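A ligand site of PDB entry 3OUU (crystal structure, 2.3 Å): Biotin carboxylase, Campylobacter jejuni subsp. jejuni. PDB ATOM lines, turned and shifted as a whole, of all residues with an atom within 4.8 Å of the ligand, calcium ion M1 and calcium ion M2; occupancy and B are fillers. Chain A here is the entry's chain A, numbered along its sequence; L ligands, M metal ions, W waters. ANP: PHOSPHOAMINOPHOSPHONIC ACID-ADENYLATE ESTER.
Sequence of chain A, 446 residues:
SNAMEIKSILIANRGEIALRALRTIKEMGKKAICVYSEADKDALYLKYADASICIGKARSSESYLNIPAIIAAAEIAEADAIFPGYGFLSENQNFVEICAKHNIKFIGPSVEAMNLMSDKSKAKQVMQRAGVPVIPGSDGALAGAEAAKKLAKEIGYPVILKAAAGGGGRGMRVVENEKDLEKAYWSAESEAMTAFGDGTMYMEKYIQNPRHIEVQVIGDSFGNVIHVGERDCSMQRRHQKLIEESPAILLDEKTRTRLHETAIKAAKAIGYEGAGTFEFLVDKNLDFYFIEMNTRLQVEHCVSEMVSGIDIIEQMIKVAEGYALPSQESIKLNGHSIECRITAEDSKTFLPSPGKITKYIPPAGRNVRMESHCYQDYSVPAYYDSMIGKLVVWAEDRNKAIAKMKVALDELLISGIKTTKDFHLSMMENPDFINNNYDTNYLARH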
ATOM      1  N   LYS A 120     -13.619  -8.230  16.797  1.00  0.00           N
ATOM      2  CA  LYS A 120     -14.636  -7.521  17.590  1.00  0.00           C
ATOM      3  C   LYS A 120     -15.511  -6.545  16.773  1.00  0.00           C
ATOM      4  O   LYS A 120     -16.680  -6.317  17.106  1.00  0.00           O
ATOM      5  CB  LYS A 120     -14.010  -6.833  18.816  1.00  0.00           C
ATOM      6  CG  LYS A 120     -13.574  -7.849  19.862  1.00  0.00           C
ATOM      7  CD  LYS A 120     -12.779  -7.256  21.001  1.00  0.00           C
ATOM      8  CE  LYS A 120     -13.565  -6.295  21.863  1.00  0.00           C
ATOM      9  NZ  LYS A 120     -12.644  -5.805  22.908  1.00  0.00           N
ATOM     10  N   ILE A 135     -23.205  -0.516  20.625  1.00  0.00           N
ATOM     11  CA  ILE A 135     -22.918   0.888  20.878  1.00  0.00           C
ATOM     12  C   ILE A 135     -22.700   1.536  19.553  1.00  0.00           C
ATOM     13  O   ILE A 135     -22.012   0.977  18.725  1.00  0.00           O
ATOM     14  CB  ILE A 135     -21.664   1.075  21.778  1.00  0.00           C
ATOM     15  CG1 ILE A 135     -21.838   0.293  23.087  1.00  0.00           C
ATOM     16  CG2 ILE A 135     -21.387   2.562  21.979  1.00  0.00           C
ATOM     17  CD1 ILE A 135     -20.731   0.486  24.090  1.00  0.00           C
ATOM     18  N   ILE A 160     -14.126   5.893  22.162  1.00  0.00           N
ATOM     19  CA  ILE A 160     -13.048   4.987  22.509  1.00  0.00           C
ATOM     20  C   ILE A 160     -12.584   4.233  21.256  1.00  0.00           C
ATOM     21  O   ILE A 160     -13.395   3.729  20.495  1.00  0.00           O
ATOM     22  CB  ILE A 160     -13.443   4.052  23.667  1.00  0.00           C
ATOM     23  CG1 ILE A 160     -12.270   3.135  24.070  1.00  0.00           C
ATOM     24  CG2 ILE A 160     -14.707   3.230  23.329  1.00  0.00           C
ATOM     25  CD1 ILE A 160     -12.521   2.416  25.405  1.00  0.00           C
ATOM     26  N   LYS A 162     -10.674   1.014  19.655  1.00  0.00           N
ATOM     27  CA  LYS A 162     -10.590  -0.362  20.109  1.00  0.00           C
ATOM     28  C   LYS A 162      -9.957  -1.229  19.007  1.00  0.00           C
ATOM     29  O   LYS A 162     -10.250  -1.049  17.813  1.00  0.00           O
ATOM     30  CB  LYS A 162     -11.979  -0.880  20.500  1.00  0.00           C
ATOM     31  CG  LYS A 162     -12.553  -0.218  21.728  1.00  0.00           C
ATOM     32  CD  LYS A 162     -13.974  -0.747  22.092  1.00  0.00           C
ATOM     33  CE  LYS A 162     -13.916  -2.017  22.978  1.00  0.00           C
ATOM     34  NZ  LYS A 162     -15.256  -2.418  23.545  1.00  0.00           N
ATOM     35  N   GLY A 166      -8.161  -7.103  19.674  1.00  0.00           N
ATOM     36  CA  GLY A 166      -7.703  -6.804  21.023  1.00  0.00           C
ATOM     37  C   GLY A 166      -8.157  -7.751  22.109  1.00  0.00           C
ATOM     38  O   GLY A 166      -9.089  -8.534  21.925  1.00  0.00           O
ATOM     39  N   GLY A 167      -7.504  -7.673  23.257  1.00  0.00           N
ATOM     40  CA  GLY A 167      -7.862  -8.456  24.429  1.00  0.00           C
ATOM     41  C   GLY A 167      -6.983  -8.022  25.596  1.00  0.00           C
ATOM     42  O   GLY A 167      -6.062  -7.237  25.421  1.00  0.00           O
ATOM     43  N   GLY A 168      -7.288  -8.527  26.787  1.00  0.00           N
ATOM     44  CA  GLY A 168      -6.504  -8.188  27.968  1.00  0.00           C
ATOM     45  C   GLY A 168      -6.599  -6.716  28.337  1.00  0.00           C
ATOM     46  O   GLY A 168      -6.067  -6.299  29.358  1.00  0.00           O
ATOM     47  N   GLY A 169      -7.257  -5.926  27.501  1.00  0.00           N
ATOM     48  CA  GLY A 169      -7.362  -4.497  27.748  1.00  0.00           C
ATOM     49  C   GLY A 169      -6.328  -3.701  26.983  1.00  0.00           C
ATOM     50  O   GLY A 169      -6.204  -2.504  27.165  1.00  0.00           O
ATOM     51  N   ARG A 170      -5.598  -4.377  26.113  1.00  0.00           N
ATOM     52  CA  ARG A 170      -4.566  -3.740  25.294  1.00  0.00           C
ATOM     53  C   ARG A 170      -5.141  -3.268  23.958  1.00  0.00           C
ATOM     54  O   ARG A 170      -6.069  -3.863  23.420  1.00  0.00           O
ATOM     55  CB  ARG A 170      -3.448  -4.764  25.051  1.00  0.00           C
ATOM     56  CG  ARG A 170      -3.196  -5.670  26.260  1.00  0.00           C
ATOM     57  CD  ARG A 170      -1.908  -6.502  26.164  1.00  0.00           C
ATOM     58  NE  ARG A 170      -1.993  -7.639  25.245  1.00  0.00           N
ATOM     59  CZ  ARG A 170      -2.638  -8.788  25.508  1.00  0.00           C
ATOM     60  NH1 ARG A 170      -3.278  -8.966  26.655  1.00  0.00           N
ATOM     61  NH2 ARG A 170      -2.642  -9.763  24.609  1.00  0.00           N
ATOM     62  N   MET A 172      -6.531  -0.225  23.285  1.00  0.00           N
ATOM     63  CA  MET A 172      -7.699   0.612  23.537  1.00  0.00           C
ATOM     64  C   MET A 172      -7.255   1.996  24.026  1.00  0.00           C
ATOM     65  O   MET A 172      -6.385   2.118  24.871  1.00  0.00           O
ATOM     66  CB  MET A 172      -8.518  -0.011  24.652  1.00  0.00           C
ATOM     67  CG  MET A 172      -9.947  -0.359  24.298  1.00  0.00           C
ATOM     68  SD  MET A 172     -10.764  -1.471  25.705  1.00  0.00           S
ATOM     69  CE  MET A 172      -9.979  -0.534  27.239  1.00  0.00           C
ATOM     70  N   GLU A 204     -16.100   3.276  19.007  1.00  0.00           N
ATOM     71  CA  GLU A 204     -17.450   3.354  19.511  1.00  0.00           C
ATOM     72  C   GLU A 204     -17.578   4.507  20.484  1.00  0.00           C
ATOM     73  O   GLU A 204     -16.578   5.039  20.960  1.00  0.00           O
ATOM     74  CB  GLU A 204     -17.952   1.999  20.078  1.00  0.00           C
ATOM     75  CG  GLU A 204     -16.962   1.226  20.914  1.00  0.00           C
ATOM     76  CD  GLU A 204     -17.501  -0.150  21.375  1.00  0.00           C
ATOM     77  OE1 GLU A 204     -18.120  -0.926  20.588  1.00  0.00           O
ATOM     78  OE2 GLU A 204     -17.245  -0.449  22.562  1.00  0.00           O
ATOM     79  N   LYS A 205     -18.808   4.915  20.748  1.00  0.00           N
ATOM     80  CA  LYS A 205     -19.034   5.957  21.724  1.00  0.00           C
ATOM     81  C   LYS A 205     -18.554   5.468  23.105  1.00  0.00           C
ATOM     82  O   LYS A 205     -18.701   4.294  23.464  1.00  0.00           O
ATOM     83  CB  LYS A 205     -20.522   6.295  21.741  1.00  0.00           C
ATOM     84  CG  LYS A 205     -20.920   7.210  22.868  1.00  0.00           C
ATOM     85  CD  LYS A 205     -20.536   8.651  22.552  1.00  0.00           C
ATOM     86  CE  LYS A 205     -20.278   9.431  23.830  1.00  0.00           C
ATOM     87  NZ  LYS A 205     -20.167  10.874  23.519  1.00  0.00           N
ATOM     88  N   TYR A 206     -17.947   6.367  23.876  1.00  0.00           N
ATOM     89  CA  TYR A 206     -17.424   5.989  25.179  1.00  0.00           C
ATOM     90  C   TYR A 206     -18.532   6.212  26.180  1.00  0.00           C
ATOM     91  O   TYR A 206     -18.960   7.351  26.417  1.00  0.00           O
ATOM     92  CB  TYR A 206     -16.200   6.821  25.535  1.00  0.00           C
ATOM     93  CG  TYR A 206     -15.554   6.507  26.863  1.00  0.00           C
ATOM     94  CD1 TYR A 206     -15.066   5.242  27.142  1.00  0.00           C
ATOM     95  CD2 TYR A 206     -15.389   7.486  27.847  1.00  0.00           C
ATOM     96  CE1 TYR A 206     -14.443   4.943  28.341  1.00  0.00           C
ATOM     97  CE2 TYR A 206     -14.773   7.201  29.064  1.00  0.00           C
ATOM     98  CZ  TYR A 206     -14.298   5.912  29.290  1.00  0.00           C
ATOM     99  OH  TYR A 206     -13.678   5.564  30.472  1.00  0.00           O
ATOM    100  N   ILE A 207     -19.023   5.137  26.779  1.00  0.00           N
ATOM    101  CA  ILE A 207     -20.083   5.280  27.772  1.00  0.00           C
ATOM    102  C   ILE A 207     -19.509   5.772  29.097  1.00  0.00           C
ATOM    103  O   ILE A 207     -18.500   5.267  29.581  1.00  0.00           O
ATOM    104  CB  ILE A 207     -20.866   3.968  27.961  1.00  0.00           C
ATOM    105  CG1 ILE A 207     -21.484   3.566  26.626  1.00  0.00           C
ATOM    106  CG2 ILE A 207     -21.979   4.156  29.000  1.00  0.00           C
ATOM    107  CD1 ILE A 207     -21.970   2.148  26.604  1.00  0.00           C
ATOM    108  N   PRO A 210     -19.872   3.375  33.065  1.00  0.00           N
ATOM    109  CA  PRO A 210     -20.670   2.198  32.745  1.00  0.00           C
ATOM    110  C   PRO A 210     -20.579   1.101  33.821  1.00  0.00           C
ATOM    111  O   PRO A 210     -19.591   0.983  34.542  1.00  0.00           O
ATOM    112  CB  PRO A 210     -19.990   1.691  31.481  1.00  0.00           C
ATOM    113  CG  PRO A 210     -18.566   1.988  31.745  1.00  0.00           C
ATOM    114  CD  PRO A 210     -18.567   3.352  32.378  1.00  0.00           C
ATOM    115  N   HIS A 212     -20.530  -3.004  33.973  1.00  0.00           N
ATOM    116  CA  HIS A 212     -20.178  -4.109  33.105  1.00  0.00           C
ATOM    117  C   HIS A 212     -20.940  -5.323  33.569  1.00  0.00           C
ATOM    118  O   HIS A 212     -20.714  -5.816  34.673  1.00  0.00           O
ATOM    119  CB  HIS A 212     -18.685  -4.386  33.218  1.00  0.00           C
ATOM    120  CG  HIS A 212     -18.178  -5.398  32.259  1.00  0.00           C
ATOM    121  ND1 HIS A 212     -18.360  -6.749  32.435  1.00  0.00           N
ATOM    122  CD2 HIS A 212     -17.438  -5.266  31.126  1.00  0.00           C
ATOM    123  CE1 HIS A 212     -17.771  -7.412  31.448  1.00  0.00           C
ATOM    124  NE2 HIS A 212     -17.201  -6.529  30.645  1.00  0.00           N
ATOM    125  N   GLN A 236     -13.426  -2.750  38.332  1.00  0.00           N
ATOM    126  CA  GLN A 236     -12.280  -3.058  37.508  1.00  0.00           C
ATOM    127  C   GLN A 236     -11.145  -2.094  37.805  1.00  0.00           C
ATOM    128  O   GLN A 236     -11.369  -0.957  38.196  1.00  0.00           O
ATOM    129  CB  GLN A 236     -12.681  -2.954  36.037  1.00  0.00           C
ATOM    130  CG  GLN A 236     -13.635  -4.045  35.566  1.00  0.00           C
ATOM    131  CD  GLN A 236     -14.097  -3.819  34.135  1.00  0.00           C
ATOM    132  OE1 GLN A 236     -13.452  -3.077  33.393  1.00  0.00           O
ATOM    133  NE2 GLN A 236     -15.224  -4.453  33.754  1.00  0.00           N
ATOM    134  N   HIS A 239      -9.315  -1.702  33.557  1.00  0.00           N
ATOM    135  CA  HIS A 239     -10.111  -2.544  32.656  1.00  0.00           C
ATOM    136  C   HIS A 239      -9.904  -4.041  32.911  1.00  0.00           C
ATOM    137  O   HIS A 239     -10.188  -4.876  32.069  1.00  0.00           O
ATOM    138  CB  HIS A 239      -9.845  -2.161  31.195  1.00  0.00           C
ATOM    139  CG  HIS A 239     -10.162  -0.726  30.909  1.00  0.00           C
ATOM    140  ND1 HIS A 239      -9.326   0.096  30.196  1.00  0.00           N
ATOM    141  CD2 HIS A 239     -11.229   0.032  31.264  1.00  0.00           C
ATOM    142  CE1 HIS A 239      -9.864   1.305  30.119  1.00  0.00           C
ATOM    143  NE2 HIS A 239     -11.025   1.294  30.747  1.00  0.00           N
ATOM    144  N   GLN A 240      -9.420  -4.345  34.114  1.00  0.00           N
ATOM    145  CA  GLN A 240      -9.126  -5.695  34.561  1.00  0.00           C
ATOM    146  C   GLN A 240     -10.115  -6.051  35.683  1.00  0.00           C
ATOM    147  O   GLN A 240     -10.365  -5.251  36.574  1.00  0.00           O
ATOM    148  CB  GLN A 240      -7.715  -5.693  35.141  1.00  0.00           C
ATOM    149  CG  GLN A 240      -6.734  -6.612  34.444  1.00  0.00           C
ATOM    150  CD  GLN A 240      -6.679  -6.409  32.949  1.00  0.00           C
ATOM    151  OE1 GLN A 240      -7.182  -7.242  32.187  1.00  0.00           O
ATOM    152  NE2 GLN A 240      -6.066  -5.318  32.526  1.00  0.00           N
ATOM    153  N   LYS A 241     -10.672  -7.263  35.650  1.00  0.00           N
ATOM    154  CA  LYS A 241     -11.642  -7.669  36.655  1.00  0.00           C
ATOM    155  C   LYS A 241     -10.991  -8.070  37.982  1.00  0.00           C
ATOM    156  O   LYS A 241      -9.958  -8.733  38.003  1.00  0.00           O
ATOM    157  CB  LYS A 241     -12.514  -8.792  36.107  1.00  0.00           C
ATOM    158  CG  LYS A 241     -13.419  -8.372  34.941  1.00  0.00           C
ATOM    159  CD  LYS A 241     -13.915  -9.583  34.180  1.00  0.00           C
ATOM    160  CE  LYS A 241     -14.829  -9.190  33.020  1.00  0.00           C
ATOM    161  NZ  LYS A 241     -15.131 -10.338  32.125  1.00  0.00           N
ATOM    162  N   GLU A 279     -20.940 -10.059  26.763  1.00  0.00           N
ATOM    163  CA  GLU A 279     -20.641  -8.883  27.577  1.00  0.00           C
ATOM    164  C   GLU A 279     -21.400  -7.629  27.154  1.00  0.00           C
ATOM    165  O   GLU A 279     -21.450  -7.280  25.961  1.00  0.00           O
ATOM    166  CB  GLU A 279     -19.142  -8.603  27.594  1.00  0.00           C
ATOM    167  CG  GLU A 279     -18.288  -9.670  28.258  1.00  0.00           C
ATOM    168  CD  GLU A 279     -16.864  -9.176  28.422  1.00  0.00           C
ATOM    169  OE1 GLU A 279     -16.665  -7.962  28.172  1.00  0.00           O
ATOM    170  OE2 GLU A 279     -15.950  -9.963  28.777  1.00  0.00           O
ATOM    171  N   LEU A 281     -22.375  -3.370  28.325  1.00  0.00           N
ATOM    172  CA  LEU A 281     -22.224  -2.232  29.217  1.00  0.00           C
ATOM    173  C   LEU A 281     -23.619  -1.687  29.462  1.00  0.00           C
ATOM    174  O   LEU A 281     -24.471  -1.760  28.590  1.00  0.00           O
ATOM    175  CB  LEU A 281     -21.279  -1.192  28.613  1.00  0.00           C
ATOM    176  CG  LEU A 281     -19.829  -1.654  28.407  1.00  0.00           C
ATOM    177  CD1 LEU A 281     -18.959  -0.548  27.806  1.00  0.00           C
ATOM    178  CD2 LEU A 281     -19.221  -2.154  29.737  1.00  0.00           C
ATOM    179  N   ILE A 291     -20.889  -5.420  23.954  1.00  0.00           N
ATOM    180  CA  ILE A 291     -19.574  -4.983  23.530  1.00  0.00           C
ATOM    181  C   ILE A 291     -18.762  -6.108  22.916  1.00  0.00           C
ATOM    182  O   ILE A 291     -17.965  -5.876  22.023  1.00  0.00           O
ATOM    183  CB  ILE A 291     -18.739  -4.247  24.620  1.00  0.00           C
ATOM    184  CG1 ILE A 291     -18.699  -5.011  25.954  1.00  0.00           C
ATOM    185  CG2 ILE A 291     -19.241  -2.823  24.819  1.00  0.00           C
ATOM    186  CD1 ILE A 291     -17.682  -4.364  26.963  1.00  0.00           C
ATOM    187  N   GLU A 292     -18.980  -7.329  23.393  1.00  0.00           N
ATOM    188  CA  GLU A 292     -18.258  -8.484  22.842  1.00  0.00           C
ATOM    189  C   GLU A 292     -18.745  -9.806  23.372  1.00  0.00           C
ATOM    190  O   GLU A 292     -19.418  -9.893  24.408  1.00  0.00           O
ATOM    191  CB  GLU A 292     -16.760  -8.362  23.088  1.00  0.00           C
ATOM    192  CG  GLU A 292     -16.343  -8.818  24.459  1.00  0.00           C
ATOM    193  CD  GLU A 292     -14.819  -8.911  24.614  1.00  0.00           C
ATOM    194  OE1 GLU A 292     -14.346  -8.873  25.759  1.00  0.00           O
ATOM    195  OE2 GLU A 292     -14.091  -9.045  23.600  1.00  0.00           O
ATOM    196  N   ASN A 294     -17.310 -13.664  24.545  1.00  0.00           N
ATOM    197  CA  ASN A 294     -16.199 -14.563  24.811  1.00  0.00           C
ATOM    198  C   ASN A 294     -16.588 -15.984  24.472  1.00  0.00           C
ATOM    199  O   ASN A 294     -17.437 -16.600  25.132  1.00  0.00           O
ATOM    200  CB  ASN A 294     -15.734 -14.472  26.256  1.00  0.00           C
ATOM    201  CG  ASN A 294     -15.175 -13.108  26.601  1.00  0.00           C
ATOM    202  OD1 ASN A 294     -14.259 -12.616  25.938  1.00  0.00           O
ATOM    203  ND2 ASN A 294     -15.745 -12.477  27.611  1.00  0.00           N
ATOM    204  N   ARG A 296     -15.655 -18.907  25.055  1.00  0.00           N
ATOM    205  CA  ARG A 296     -14.972 -19.832  25.940  1.00  0.00           C
ATOM    206  C   ARG A 296     -15.518 -19.648  27.356  1.00  0.00           C
ATOM    207  O   ARG A 296     -16.202 -18.670  27.640  1.00  0.00           O
ATOM    208  CB  ARG A 296     -13.466 -19.531  25.958  1.00  0.00           C
ATOM    209  CG  ARG A 296     -13.134 -18.073  26.337  1.00  0.00           C
ATOM    210  CD  ARG A 296     -11.651 -17.885  26.712  1.00  0.00           C
ATOM    211  NE  ARG A 296     -11.308 -16.462  26.801  1.00  0.00           N
ATOM    212  CZ  ARG A 296     -11.775 -15.633  27.728  1.00  0.00           C
ATOM    213  NH1 ARG A 296     -11.431 -14.343  27.719  1.00  0.00           N
ATOM    214  NH2 ARG A 296     -12.591 -16.076  28.674  1.00  0.00           N
ATOM    215  N   THR A 440     -16.938   0.991  36.272  1.00  0.00           N
ATOM    216  CA  THR A 440     -15.638   0.585  35.769  1.00  0.00           C
ATOM    217  C   THR A 440     -14.511   1.583  36.037  1.00  0.00           C
ATOM    218  O   THR A 440     -13.349   1.231  35.975  1.00  0.00           O
ATOM    219  CB  THR A 440     -15.729   0.292  34.271  1.00  0.00           C
ATOM    220  OG1 THR A 440     -16.153   1.479  33.599  1.00  0.00           O
ATOM    221  CG2 THR A 440     -16.775  -0.844  34.020  1.00  0.00           C
HETATM  222  PG  ANP L   1     -10.769  -8.514  28.030  1.00  0.00           P
HETATM  223  O1G ANP L   1     -11.767  -9.656  28.169  1.00  0.00           O
HETATM  224  O2G ANP L   1     -10.127  -8.181  29.333  1.00  0.00           O
HETATM  225  O3G ANP L   1      -9.669  -9.008  27.003  1.00  0.00           O
HETATM  226  PB  ANP L   1     -10.880  -6.426  26.074  1.00  0.00           P
HETATM  227  O1B ANP L   1     -11.490  -7.514  25.088  1.00  0.00           O
HETATM  228  O2B ANP L   1      -9.363  -6.090  25.997  1.00  0.00           O
HETATM  229  N3B ANP L   1     -11.495  -7.105  27.466  1.00  0.00           N
HETATM  230  PA  ANP L   1     -13.349  -5.060  26.162  1.00  0.00           P
HETATM  231  O1A ANP L   1     -13.943  -6.241  26.814  1.00  0.00           O
HETATM  232  O2A ANP L   1     -14.070  -4.685  24.919  1.00  0.00           O
HETATM  233  O3A ANP L   1     -11.834  -5.221  25.838  1.00  0.00           O
HETATM  234  O5' ANP L   1     -13.472  -3.847  27.172  1.00  0.00           O
HETATM  235  C5' ANP L   1     -12.951  -3.881  28.526  1.00  0.00           C
HETATM  236  C4' ANP L   1     -13.316  -2.771  29.430  1.00  0.00           C
HETATM  237  O4' ANP L   1     -13.091  -1.539  28.818  1.00  0.00           O
HETATM  238  C3' ANP L   1     -14.778  -2.821  29.626  1.00  0.00           C
HETATM  239  O3' ANP L   1     -15.095  -3.694  30.640  1.00  0.00           O
HETATM  240  C2' ANP L   1     -15.120  -1.463  29.905  1.00  0.00           C
HETATM  241  O2' ANP L   1     -14.675  -1.133  31.172  1.00  0.00           O
HETATM  242  C1' ANP L   1     -14.265  -0.724  28.973  1.00  0.00           C
HETATM  243  N9  ANP L   1     -14.956  -0.390  27.727  1.00  0.00           N
HETATM  244  C8  ANP L   1     -14.942  -1.071  26.549  1.00  0.00           C
HETATM  245  N7  ANP L   1     -15.712  -0.427  25.645  1.00  0.00           N
HETATM  246  C5  ANP L   1     -16.238   0.667  26.255  1.00  0.00           C
HETATM  247  C6  ANP L   1     -17.104   1.681  25.829  1.00  0.00           C
HETATM  248  N6  ANP L   1     -17.657   1.737  24.454  1.00  0.00           N
HETATM  249  N1  ANP L   1     -17.436   2.649  26.697  1.00  0.00           N
HETATM  250  C2  ANP L   1     -16.985   2.663  27.964  1.00  0.00           C
HETATM  251  N3  ANP L   1     -16.149   1.694  28.406  1.00  0.00           N
HETATM  252  C4  ANP L   1     -15.768   0.697  27.584  1.00  0.00           C
HETATM  253 CA    CA M   1     -12.024  -9.874  25.099  1.00  0.00          CA
HETATM  254 CA    CA M   2     -14.077  -8.174  28.014  1.00  0.00          CA
HETATM  255  O   HOH W   1     -10.900  -9.923  22.778  1.00  0.00           O
HETATM  256  O   HOH W   2     -15.378   2.065  31.097  1.00  0.00           O
HETATM  257  O   HOH W   3     -12.047  -7.323  31.809  1.00  0.00           O
HETATM  258  O   HOH W   4     -12.737 -11.895  30.032  1.00  0.00           O
HETATM  259  O   HOH W   5     -13.872  -6.904  30.290  1.00  0.00           O
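O2A of the ligand is in salt-bridge range of NZ of Lys 120 (2.7 Å). The side-chain amino group (NZ) of Lys 162 is in salt-bridge range of an oxygen (O2A) of the ligand (2.9 Å). N of Ile 207 is in hydrogen-bond range of N1 of the ligand. The backbone NH of Gly 169 sits at hydrogen-bond distance from an oxygen (O2B) of the ligand. The backbone carbonyl oxygen of Lys 205 lies within hydrogen-bond range of a nitrogen (N6) of the ligand, 2.9 Å away. N6 of the ligand is in hydrogen-bond range of OE2 of Glu 204 (2.9 Å). OE1 of Gln 236 sits at hydrogen-bond distance from O2' of the ligand (3.2 Å). The backbone NH (N) of Gly 168 lies within hydrogen-bond range of an oxygen (O3G) of the ligand (2.4 Å).
The backbone carbonyl oxygen of Glu 204 is in hydrogen-bond range of the backbone NH of Ile 160, at 2.9 Å. OE2 of Glu 279 lies close to ND2 of Asn 294 (2.8 Å). OE2 of Glu 204 is in salt-bridge range of NZ of Lys 162, at 3.0 Å. OE2 of Glu 292 lies close to NZ of Lys 120 (3.6 Å). The side-chain carboxylate (OE1) of Glu 279 lies close to a ring nitrogen (NE2) of His 212. The backbone NH of Thr 440 sits at hydrogen-bond distance from the backbone carbonyl oxygen of Pro 210, at 3.2 Å. The side-chain carboxylate (OE2) of Glu 279 lies close to the side-chain amino group (NZ) of Lys 241 (3.5 Å). The backbone NH of Ile 291 is in hydrogen-bond range of the backbone carbonyl oxygen of Glu 279, at 2.8 Å.
CD1 of Ile 135 touches N6 of the ligand, 3.3 Å away. Ile 160 touches the ligand. Gly 167 touches the ligand. CE of Met 172 touches O4' of the ligand (3.6 Å). Tyr 206 touches the ligand (CD1 to C2, 3.3 Å). His 212 touches the ligand (CD2 to O3', 2.9 Å). CD2 of His 239 touches O4' of the ligand (3.5 Å). CD1 of Leu 281 touches C5 of the ligand, 3.4 Å away. Thr 440 touches the ligand. Hydrophobic or aromatic side chains within 4 Å of the ligand: Ile 135, Ile 160, Met 172, Tyr 206, Ile 207, His 212, His 239 and Leu 281. Within 4 Å of the ligand: Lys 120, Ile 135, Ile 160, Lys 162, Gly 167, Gly 168, Gly 169, Met 172, Glu 204, Lys 205, Tyr 206, Ile 207, His 212, Gln 236, His 239, Glu 279, Leu 281, Glu 292 and Thr 440.
OD1 of Asn 294 touches calcium ion M1, 3.6 Å away. Within 4 Å of calcium ion M1: Glu 292 and Asn 294. The nearest printed residue that does not touch calcium ion M1 is Gly 167 (4.4 Å).
Of the 27 residues printed, 2 come within 4 Å of calcium ion M2.
Calcium ion M1 is bound by O1B of the ligand (2.4 Å). Water W1 is bound to calcium ion M1. Calcium ion M1 is bound by OE1 of Glu 292 (2.6 Å). Calcium ion M1 is bound by OE2 of Glu 292, 2.7 Å away. Calcium ion M1 has four donor atoms within binding distance. Slightly farther from calcium ion M1 lies O1G of the ligand (3.1 Å). Slightly farther from calcium ion M1 lies an oxygen (O3G) of the ligand (3.1 Å).
Calcium ion M2 is bound by an oxygen (O1A) of the ligand (2.3 Å), the side-chain carboxylate (OE1) of Glu 292 (2.4 Å), the side-chain carboxylate (OE1) of Glu 279 (2.6 Å), water W5 (2.6 Å), the side-chain carboxylate (OE2) of Glu 279 (2.7 Å), an oxygen (O1G) of the ligand (2.7 Å) and a nitrogen (N3B) of the ligand (2.8 Å). Calcium ion M2 has seven donor atoms within binding distance.
Water W5 lies within hydrogen-bond range of NE2 of His 212 (3.4 Å) and O3' of the ligand (3.5 Å). Water W2 lies within hydrogen-bond range of the side-chain hydroxyl (OG1) of Thr 440 (2.7 Å) and a nitrogen (N3) of the ligand (2.8 Å). Water W3 bridges the backbone carbonyl oxygen of His 239 (3.1 Å) and an oxygen (O2G) of the ligand (3.2 Å).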
